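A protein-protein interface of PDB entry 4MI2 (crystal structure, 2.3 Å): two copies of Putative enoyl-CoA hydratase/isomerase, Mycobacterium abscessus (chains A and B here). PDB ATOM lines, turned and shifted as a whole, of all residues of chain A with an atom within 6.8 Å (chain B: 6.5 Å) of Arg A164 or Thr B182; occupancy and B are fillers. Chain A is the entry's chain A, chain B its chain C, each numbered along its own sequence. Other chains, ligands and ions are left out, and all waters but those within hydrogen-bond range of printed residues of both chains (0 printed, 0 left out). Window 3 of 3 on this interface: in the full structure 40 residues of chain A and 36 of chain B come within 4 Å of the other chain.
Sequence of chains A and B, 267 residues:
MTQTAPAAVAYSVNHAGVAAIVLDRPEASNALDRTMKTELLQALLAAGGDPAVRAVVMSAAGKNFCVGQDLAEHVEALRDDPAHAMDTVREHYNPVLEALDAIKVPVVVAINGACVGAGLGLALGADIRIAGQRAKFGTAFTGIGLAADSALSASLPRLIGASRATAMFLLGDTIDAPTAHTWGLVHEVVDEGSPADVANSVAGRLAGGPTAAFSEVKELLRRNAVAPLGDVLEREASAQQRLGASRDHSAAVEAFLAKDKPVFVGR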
ATOM      1  N   LEU A 156       8.693   2.880  -6.487  1.00  0.00           N
ATOM      2  CA  LEU A 156       8.066   3.248  -7.762  1.00  0.00           C
ATOM      3  C   LEU A 156       8.657   4.538  -8.365  1.00  0.00           C
ATOM      4  O   LEU A 156       9.129   4.508  -9.500  1.00  0.00           O
ATOM      5  CB  LEU A 156       6.536   3.330  -7.643  1.00  0.00           C
ATOM      6  CG  LEU A 156       5.760   3.498  -8.958  1.00  0.00           C
ATOM      7  CD1 LEU A 156       6.040   2.356  -9.926  1.00  0.00           C
ATOM      8  CD2 LEU A 156       4.265   3.598  -8.681  1.00  0.00           C
ATOM      9  N   PRO A 157       8.648   5.666  -7.618  1.00  0.00           N
ATOM     10  CA  PRO A 157       9.233   6.876  -8.200  1.00  0.00           C
ATOM     11  C   PRO A 157      10.724   6.778  -8.505  1.00  0.00           C
ATOM     12  O   PRO A 157      11.216   7.468  -9.394  1.00  0.00           O
ATOM     13  CB  PRO A 157       8.969   7.959  -7.135  1.00  0.00           C
ATOM     14  CG  PRO A 157       8.642   7.210  -5.891  1.00  0.00           C
ATOM     15  CD  PRO A 157       7.950   5.965  -6.359  1.00  0.00           C
ATOM     16  N   ILE A 160      10.645   4.929 -12.078  1.00  0.00           N
ATOM     17  CA  ILE A 160       9.993   5.591 -13.212  1.00  0.00           C
ATOM     18  C   ILE A 160       9.885   7.112 -13.094  1.00  0.00           C
ATOM     19  O   ILE A 160       9.340   7.750 -13.989  1.00  0.00           O
ATOM     20  CB  ILE A 160       8.585   5.002 -13.505  1.00  0.00           C
ATOM     21  CG1 ILE A 160       7.590   5.305 -12.384  1.00  0.00           C
ATOM     22  CG2 ILE A 160       8.690   3.505 -13.765  1.00  0.00           C
ATOM     23  CD1 ILE A 160       6.178   4.839 -12.686  1.00  0.00           C
ATOM     24  N   GLY A 161      10.406   7.682 -12.009  1.00  0.00           N
ATOM     25  CA  GLY A 161      10.301   9.114 -11.754  1.00  0.00           C
ATOM     26  C   GLY A 161       9.070   9.477 -10.942  1.00  0.00           C
ATOM     27  O   GLY A 161       8.079   8.753 -10.951  1.00  0.00           O
ATOM     28  N   ALA A 162       9.153  10.606 -10.240  1.00  0.00           N
ATOM     29  CA  ALA A 162       8.065  11.126  -9.390  1.00  0.00           C
ATOM     30  C   ALA A 162       6.786  11.432 -10.169  1.00  0.00           C
ATOM     31  O   ALA A 162       5.686  11.159  -9.696  1.00  0.00           O
ATOM     32  CB  ALA A 162       8.522  12.391  -8.652  1.00  0.00           C
ATOM     33  N   SER A 163       6.924  12.015 -11.347  1.00  0.00           N
ATOM     34  CA  SER A 163       5.741  12.383 -12.114  1.00  0.00           C
ATOM     35  C   SER A 163       4.861  11.195 -12.524  1.00  0.00           C
ATOM     36  O   SER A 163       3.652  11.235 -12.335  1.00  0.00           O
ATOM     37  CB  SER A 163       6.120  13.154 -13.357  1.00  0.00           C
ATOM     38  OG  SER A 163       4.944  13.727 -13.893  1.00  0.00           O
ATOM     39  N   ARG A 164       5.454  10.152 -13.100  1.00  0.00           N
ATOM     40  CA  ARG A 164       4.656   8.994 -13.520  1.00  0.00           C
ATOM     41  C   ARG A 164       4.208   8.123 -12.339  1.00  0.00           C
ATOM     42  O   ARG A 164       3.131   7.517 -12.383  1.00  0.00           O
ATOM     43  CB  ARG A 164       5.411   8.177 -14.561  1.00  0.00           C
ATOM     44  CG  ARG A 164       5.487   8.902 -15.897  1.00  0.00           C
ATOM     45  CD  ARG A 164       6.614   8.380 -16.762  1.00  0.00           C
ATOM     46  NE  ARG A 164       6.586   8.991 -18.092  1.00  0.00           N
ATOM     47  CZ  ARG A 164       7.543   8.855 -19.001  1.00  0.00           C
ATOM     48  NH1 ARG A 164       7.424   9.453 -20.186  1.00  0.00           N
ATOM     49  NH2 ARG A 164       8.627   8.135 -18.727  1.00  0.00           N
ATOM     50  N   ALA A 165       5.028   8.084 -11.287  1.00  0.00           N
ATOM     51  CA  ALA A 165       4.650   7.431 -10.032  1.00  0.00           C
ATOM     52  C   ALA A 165       3.410   8.092  -9.420  1.00  0.00           C
ATOM     53  O   ALA A 165       2.448   7.411  -9.038  1.00  0.00           O
ATOM     54  CB  ALA A 165       5.818   7.472  -9.049  1.00  0.00           C
ATOM     55  N   THR A 166       3.433   9.423  -9.366  1.00  0.00           N
ATOM     56  CA  THR A 166       2.327  10.198  -8.839  1.00  0.00           C
ATOM     57  C   THR A 166       1.054   9.903  -9.632  1.00  0.00           C
ATOM     58  O   THR A 166       0.007   9.617  -9.047  1.00  0.00           O
ATOM     59  CB  THR A 166       2.641  11.716  -8.885  1.00  0.00           C
ATOM     60  OG1 THR A 166       3.799  11.987  -8.091  1.00  0.00           O
ATOM     61  CG2 THR A 166       1.484  12.535  -8.351  1.00  0.00           C
ATOM     62  N   ALA A 167       1.152   9.958 -10.960  1.00  0.00           N
ATOM     63  CA  ALA A 167       0.021   9.631 -11.836  1.00  0.00           C
ATOM     64  C   ALA A 167      -0.565   8.242 -11.552  1.00  0.00           C
ATOM     65  O   ALA A 167      -1.776   8.092 -11.414  1.00  0.00           O
ATOM     66  CB  ALA A 167       0.424   9.739 -13.301  1.00  0.00           C
ATOM     67  N   MET A 168       0.289   7.231 -11.450  1.00  0.00           N
ATOM     68  CA  MET A 168      -0.195   5.877 -11.177  1.00  0.00           C
ATOM     69  C   MET A 168      -0.933   5.805  -9.842  1.00  0.00           C
ATOM     70  O   MET A 168      -1.940   5.119  -9.745  1.00  0.00           O
ATOM     71  CB  MET A 168       0.951   4.865 -11.193  1.00  0.00           C
ATOM     72  CG  MET A 168       1.508   4.589 -12.579  1.00  0.00           C
ATOM     73  SD  MET A 168       2.787   3.322 -12.546  1.00  0.00           S
ATOM     74  CE  MET A 168       1.862   1.887 -12.032  1.00  0.00           C
ATOM     75  N   PHE A 169      -0.432   6.507  -8.825  1.00  0.00           N
ATOM     76  CA  PHE A 169      -1.058   6.529  -7.494  1.00  0.00           C
ATOM     77  C   PHE A 169      -2.381   7.304  -7.473  1.00  0.00           C
ATOM     78  O   PHE A 169      -3.359   6.844  -6.877  1.00  0.00           O
ATOM     79  CB  PHE A 169      -0.109   7.139  -6.437  1.00  0.00           C
ATOM     80  CG  PHE A 169       0.816   6.143  -5.785  1.00  0.00           C
ATOM     81  CD1 PHE A 169       0.311   5.131  -4.976  1.00  0.00           C
ATOM     82  CD2 PHE A 169       2.195   6.238  -5.949  1.00  0.00           C
ATOM     83  CE1 PHE A 169       1.164   4.221  -4.360  1.00  0.00           C
ATOM     84  CE2 PHE A 169       3.054   5.330  -5.341  1.00  0.00           C
ATOM     85  CZ  PHE A 169       2.537   4.323  -4.542  1.00  0.00           C
ATOM     86  N   THR A 182       9.213   0.854 -21.439  1.00  0.00           N
ATOM     87  CA  THR A 182       9.591   2.203 -21.886  1.00  0.00           C
ATOM     88  C   THR A 182       9.842   3.149 -20.710  1.00  0.00           C
ATOM     89  O   THR A 182      10.729   4.000 -20.768  1.00  0.00           O
ATOM     90  CB  THR A 182       8.513   2.809 -22.807  1.00  0.00           C
ATOM     91  OG1 THR A 182       8.267   1.909 -23.892  1.00  0.00           O
ATOM     92  CG2 THR A 182       8.952   4.194 -23.370  1.00  0.00           C
ATOM     93  N   TRP A 183       9.076   2.980 -19.640  1.00  0.00           N
ATOM     94  CA  TRP A 183       9.191   3.834 -18.456  1.00  0.00           C
ATOM     95  C   TRP A 183      10.349   3.455 -17.523  1.00  0.00           C
ATOM     96  O   TRP A 183      10.694   4.227 -16.633  1.00  0.00           O
ATOM     97  CB  TRP A 183       7.872   3.810 -17.683  1.00  0.00           C
ATOM     98  CG  TRP A 183       6.777   4.626 -18.322  1.00  0.00           C
ATOM     99  CD1 TRP A 183       6.787   5.194 -19.570  1.00  0.00           C
ATOM    100  CD2 TRP A 183       5.506   4.957 -17.741  1.00  0.00           C
ATOM    101  NE1 TRP A 183       5.611   5.862 -19.790  1.00  0.00           N
ATOM    102  CE2 TRP A 183       4.807   5.738 -18.687  1.00  0.00           C
ATOM    103  CE3 TRP A 183       4.894   4.674 -16.514  1.00  0.00           C
ATOM    104  CZ2 TRP A 183       3.519   6.233 -18.449  1.00  0.00           C
ATOM    105  CZ3 TRP A 183       3.613   5.172 -16.273  1.00  0.00           C
ATOM    106  CH2 TRP A 183       2.937   5.939 -17.241  1.00  0.00           C
ATOM    107  N   GLY A 184      10.941   2.281 -17.717  1.00  0.00           N
ATOM    108  CA  GLY A 184      12.043   1.818 -16.875  1.00  0.00           C
ATOM    109  C   GLY A 184      11.619   0.955 -15.684  1.00  0.00           C
ATOM    110  O   GLY A 184      12.430   0.671 -14.793  1.00  0.00           O
ATOM    111  N   ARG B 129      -0.096  17.297 -15.302  1.00  0.00           N
ATOM    112  CA  ARG B 129       0.131  18.331 -16.301  1.00  0.00           C
ATOM    113  C   ARG B 129      -0.462  17.862 -17.621  1.00  0.00           C
ATOM    114  O   ARG B 129      -0.106  16.793 -18.127  1.00  0.00           O
ATOM    115  CB  ARG B 129       1.629  18.623 -16.453  1.00  0.00           C
ATOM    116  CG  ARG B 129       2.214  19.426 -15.296  1.00  0.00           C
ATOM    117  CD  ARG B 129       3.737  19.406 -15.277  1.00  0.00           C
ATOM    118  NE  ARG B 129       4.224  18.093 -14.887  1.00  0.00           N
ATOM    119  CZ  ARG B 129       4.344  17.668 -13.634  1.00  0.00           C
ATOM    120  NH1 ARG B 129       4.045  18.462 -12.615  1.00  0.00           N
ATOM    121  NH2 ARG B 129       4.777  16.437 -13.402  1.00  0.00           N
ATOM    122  N   ARG B 164      18.946  16.518 -19.352  1.00  0.00           N
ATOM    123  CA  ARG B 164      18.034  17.294 -20.180  1.00  0.00           C
ATOM    124  C   ARG B 164      17.672  18.647 -19.568  1.00  0.00           C
ATOM    125  O   ARG B 164      17.534  19.630 -20.295  1.00  0.00           O
ATOM    126  CB  ARG B 164      16.776  16.491 -20.485  1.00  0.00           C
ATOM    127  CG  ARG B 164      17.018  15.458 -21.562  1.00  0.00           C
ATOM    128  CD  ARG B 164      15.932  14.401 -21.577  1.00  0.00           C
ATOM    129  NE  ARG B 164      16.234  13.377 -22.575  1.00  0.00           N
ATOM    130  CZ  ARG B 164      15.665  12.179 -22.644  1.00  0.00           C
ATOM    131  NH1 ARG B 164      14.727  11.818 -21.768  1.00  0.00           N
ATOM    132  NH2 ARG B 164      16.037  11.345 -23.608  1.00  0.00           N
ATOM    133  N   ALA B 177       5.323  20.072 -27.282  1.00  0.00           N
ATOM    134  CA  ALA B 177       4.471  19.222 -26.462  1.00  0.00           C
ATOM    135  C   ALA B 177       4.817  17.733 -26.546  1.00  0.00           C
ATOM    136  O   ALA B 177       5.002  17.102 -25.513  1.00  0.00           O
ATOM    137  CB  ALA B 177       3.007  19.457 -26.795  1.00  0.00           C
ATOM    138  N   PRO B 178       4.918  17.165 -27.763  1.00  0.00           N
ATOM    139  CA  PRO B 178       5.234  15.730 -27.825  1.00  0.00           C
ATOM    140  C   PRO B 178       6.608  15.384 -27.253  1.00  0.00           C
ATOM    141  O   PRO B 178       6.796  14.285 -26.729  1.00  0.00           O
ATOM    142  CB  PRO B 178       5.168  15.402 -29.326  1.00  0.00           C
ATOM    143  CG  PRO B 178       5.240  16.708 -30.032  1.00  0.00           C
ATOM    144  CD  PRO B 178       4.675  17.738 -29.098  1.00  0.00           C
ATOM    145  N   THR B 179       7.563  16.304 -27.343  1.00  0.00           N
ATOM    146  CA  THR B 179       8.859  16.094 -26.701  1.00  0.00           C
ATOM    147  C   THR B 179       8.703  16.115 -25.182  1.00  0.00           C
ATOM    148  O   THR B 179       9.248  15.254 -24.486  1.00  0.00           O
ATOM    149  CB  THR B 179       9.890  17.158 -27.118  1.00  0.00           C
ATOM    150  OG1 THR B 179      10.002  17.180 -28.544  1.00  0.00           O
ATOM    151  CG2 THR B 179      11.254  16.852 -26.521  1.00  0.00           C
ATOM    152  N   ALA B 180       7.950  17.090 -24.677  1.00  0.00           N
ATOM    153  CA  ALA B 180       7.689  17.201 -23.241  1.00  0.00           C
ATOM    154  C   ALA B 180       7.017  15.938 -22.707  1.00  0.00           C
ATOM    155  O   ALA B 180       7.339  15.463 -21.611  1.00  0.00           O
ATOM    156  CB  ALA B 180       6.828  18.422 -22.951  1.00  0.00           C
ATOM    157  N   HIS B 181       6.090  15.406 -23.499  1.00  0.00           N
ATOM    158  CA  HIS B 181       5.381  14.183 -23.160  1.00  0.00           C
ATOM    159  C   HIS B 181       6.351  13.015 -23.041  1.00  0.00           C
ATOM    160  O   HIS B 181       6.364  12.314 -22.031  1.00  0.00           O
ATOM    161  CB  HIS B 181       4.329  13.884 -24.226  1.00  0.00           C
ATOM    162  CG  HIS B 181       3.363  12.808 -23.842  1.00  0.00           C
ATOM    163  ND1 HIS B 181       3.098  11.722 -24.650  1.00  0.00           N
ATOM    164  CD2 HIS B 181       2.600  12.650 -22.736  1.00  0.00           C
ATOM    165  CE1 HIS B 181       2.206  10.946 -24.061  1.00  0.00           C
ATOM    166  NE2 HIS B 181       1.888  11.485 -22.896  1.00  0.00           N
ATOM    167  N   THR B 182       7.172  12.830 -24.070  1.00  0.00           N
ATOM    168  CA  THR B 182       8.125  11.729 -24.118  1.00  0.00           C
ATOM    169  C   THR B 182       9.184  11.861 -23.023  1.00  0.00           C
ATOM    170  O   THR B 182       9.644  10.862 -22.475  1.00  0.00           O
ATOM    171  CB  THR B 182       8.806  11.653 -25.505  1.00  0.00           C
ATOM    172  OG1 THR B 182       7.824  11.321 -26.494  1.00  0.00           O
ATOM    173  CG2 THR B 182       9.921  10.601 -25.532  1.00  0.00           C
ATOM    174  N   TRP B 183       9.552  13.097 -22.708  1.00  0.00           N
ATOM    175  CA  TRP B 183      10.549  13.379 -21.686  1.00  0.00           C
ATOM    176  C   TRP B 183       9.996  13.270 -20.265  1.00  0.00           C
ATOM    177  O   TRP B 183      10.767  13.205 -19.313  1.00  0.00           O
ATOM    178  CB  TRP B 183      11.127  14.777 -21.908  1.00  0.00           C
ATOM    179  CG  TRP B 183      12.168  14.839 -22.966  1.00  0.00           C
ATOM    180  CD1 TRP B 183      12.450  13.887 -23.902  1.00  0.00           C
ATOM    181  CD2 TRP B 183      13.068  15.922 -23.210  1.00  0.00           C
ATOM    182  NE1 TRP B 183      13.480  14.306 -24.703  1.00  0.00           N
ATOM    183  CE2 TRP B 183      13.876  15.554 -24.303  1.00  0.00           C
ATOM    184  CE3 TRP B 183      13.274  17.166 -22.609  1.00  0.00           C
ATOM    185  CZ2 TRP B 183      14.882  16.392 -24.809  1.00  0.00           C
ATOM    186  CZ3 TRP B 183      14.267  17.997 -23.113  1.00  0.00           C
ATOM    187  CH2 TRP B 183      15.057  17.606 -24.201  1.00  0.00           C
ATOM    188  N   GLY B 184       8.671  13.274 -20.119  1.00  0.00           N
ATOM    189  CA  GLY B 184       8.026  13.148 -18.800  1.00  0.00           C
ATOM    190  C   GLY B 184       7.699  14.470 -18.130  1.00  0.00           C
ATOM    191  O   GLY B 184       7.391  14.511 -16.942  1.00  0.00           O
ATOM    192  N   LEU B 185       7.761  15.553 -18.895  1.00  0.00           N
ATOM    193  CA  LEU B 185       7.466  16.885 -18.373  1.00  0.00           C
ATOM    194  C   LEU B 185       5.957  17.081 -18.196  1.00  0.00           C
ATOM    195  O   LEU B 185       5.525  17.758 -17.263  1.00  0.00           O
ATOM    196  CB  LEU B 185       8.034  17.958 -19.306  1.00  0.00           C
ATOM    197  CG  LEU B 185       8.143  19.372 -18.729  1.00  0.00           C
ATOM    198  CD1 LEU B 185       9.203  19.430 -17.643  1.00  0.00           C
ATOM    199  CD2 LEU B 185       8.483  20.365 -19.817  1.00  0.00           C
ATOM    200  N   VAL B 186       5.169  16.494 -19.098  1.00  0.00           N
ATOM    201  CA  VAL B 186       3.708  16.492 -18.987  1.00  0.00           C
ATOM    202  C   VAL B 186       3.176  15.069 -19.112  1.00  0.00           C
ATOM    203  O   VAL B 186       3.841  14.203 -19.679  1.00  0.00           O
ATOM    204  CB  VAL B 186       3.057  17.388 -20.057  1.00  0.00           C
ATOM    205  CG1 VAL B 186       3.548  18.823 -19.913  1.00  0.00           C
ATOM    206  CG2 VAL B 186       3.346  16.861 -21.455  1.00  0.00           C
ATOM    207  N   HIS B 187       1.977  14.835 -18.586  1.00  0.00           N
ATOM    208  CA  HIS B 187       1.374  13.495 -18.598  1.00  0.00           C
ATOM    209  C   HIS B 187       0.594  13.188 -19.882  1.00  0.00           C
ATOM    210  O   HIS B 187       0.532  12.033 -20.301  1.00  0.00           O
ATOM    211  CB  HIS B 187       0.476  13.304 -17.370  1.00  0.00           C
ATOM    212  CG  HIS B 187       1.226  13.342 -16.071  1.00  0.00           C
ATOM    213  ND1 HIS B 187       1.512  14.517 -15.411  1.00  0.00           N
ATOM    214  CD2 HIS B 187       1.770  12.352 -15.322  1.00  0.00           C
ATOM    215  CE1 HIS B 187       2.189  14.253 -14.310  1.00  0.00           C
ATOM    216  NE2 HIS B 187       2.363  12.946 -14.234  1.00  0.00           N
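Arg A164 touches Thr B182, but with the chains exchanged Thr A182 does not touch Arg B164 (8.8 Å).
Arg A164 touches Gly B184, but with the chains exchanged Gly A184 does not touch Arg B164 (11.0 Å).
Of the 7 pairs that touch across the chains among the printed residues, none has its exchanged pair printed and touching as well.
Printed residues of chain B within 4 Å of Arg A164: His B181 (3.6 Å), Thr B182 (3.5 Å) and Gly B184 (3.99 Å).
Thr B182 touches one residue of chain A.
Of the printed residues of chain B, Ser A163 touches Arg B129, Gly B184 and His B187.
Of the printed residues of chain A, His B181 touches Arg A164.
Of the printed residues of chain A, Gly B184 touches Ser A163 and Arg A164.
The nearest printed residue of chain B that does not touch Arg A164 is His B187 (4.3 Å).
The nearest printed residue of chain A that does not touch Thr B182 is Thr A182 (6.8 Å).
The nearest printed residue of chain A that does not touch Gly B184 is Ile A160 (7.3 Å).
Of the 15 printed residues of chain A, 3 touch a printed residue of chain B.
Hydrophobic or aromatic side chains of chain A within 4 Å of the printed part of chain B: Ala A167.
Hydrophobic or aromatic side chains of chain B within 4 Å of the printed part of chain A: His B187.
Among the printed residues, 7 pairs touch across the chains.
The side-chain hydroxyl of Ser A163 sits at hydrogen-bond distance from the guanidinium group of Arg B129 (2.8 Å).
The side-chain hydroxyl of Ser A163 lies within hydrogen-bond range of a ring nitrogen (NE2) of His B187 (2.7 Å).
The backbone carbonyl oxygen (O) of Thr B182 sits at hydrogen-bond distance from the guanidinium group (NH1) of Arg A164 (3.5 Å).
The backbone carbonyl oxygen of Leu B185 lies within hydrogen-bond range of the guanidinium group of Arg B129 (2.7 Å).
O of Arg B129 sits at hydrogen-bond distance from N of His B187.
O of Pro B178 sits at hydrogen-bond distance from OG1 of Thr B182 (3.1 Å).
A ring nitrogen (NE2) of His B181 is in hydrogen-bond range of the backbone carbonyl oxygen of His B187, 3.0 Å away.
Among the printed residues, merely in contact across the chains: Ser A163 with Gly B184, Arg A164 with His B181, Arg A164 with Gly B184 and Ala A167 with His B187.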
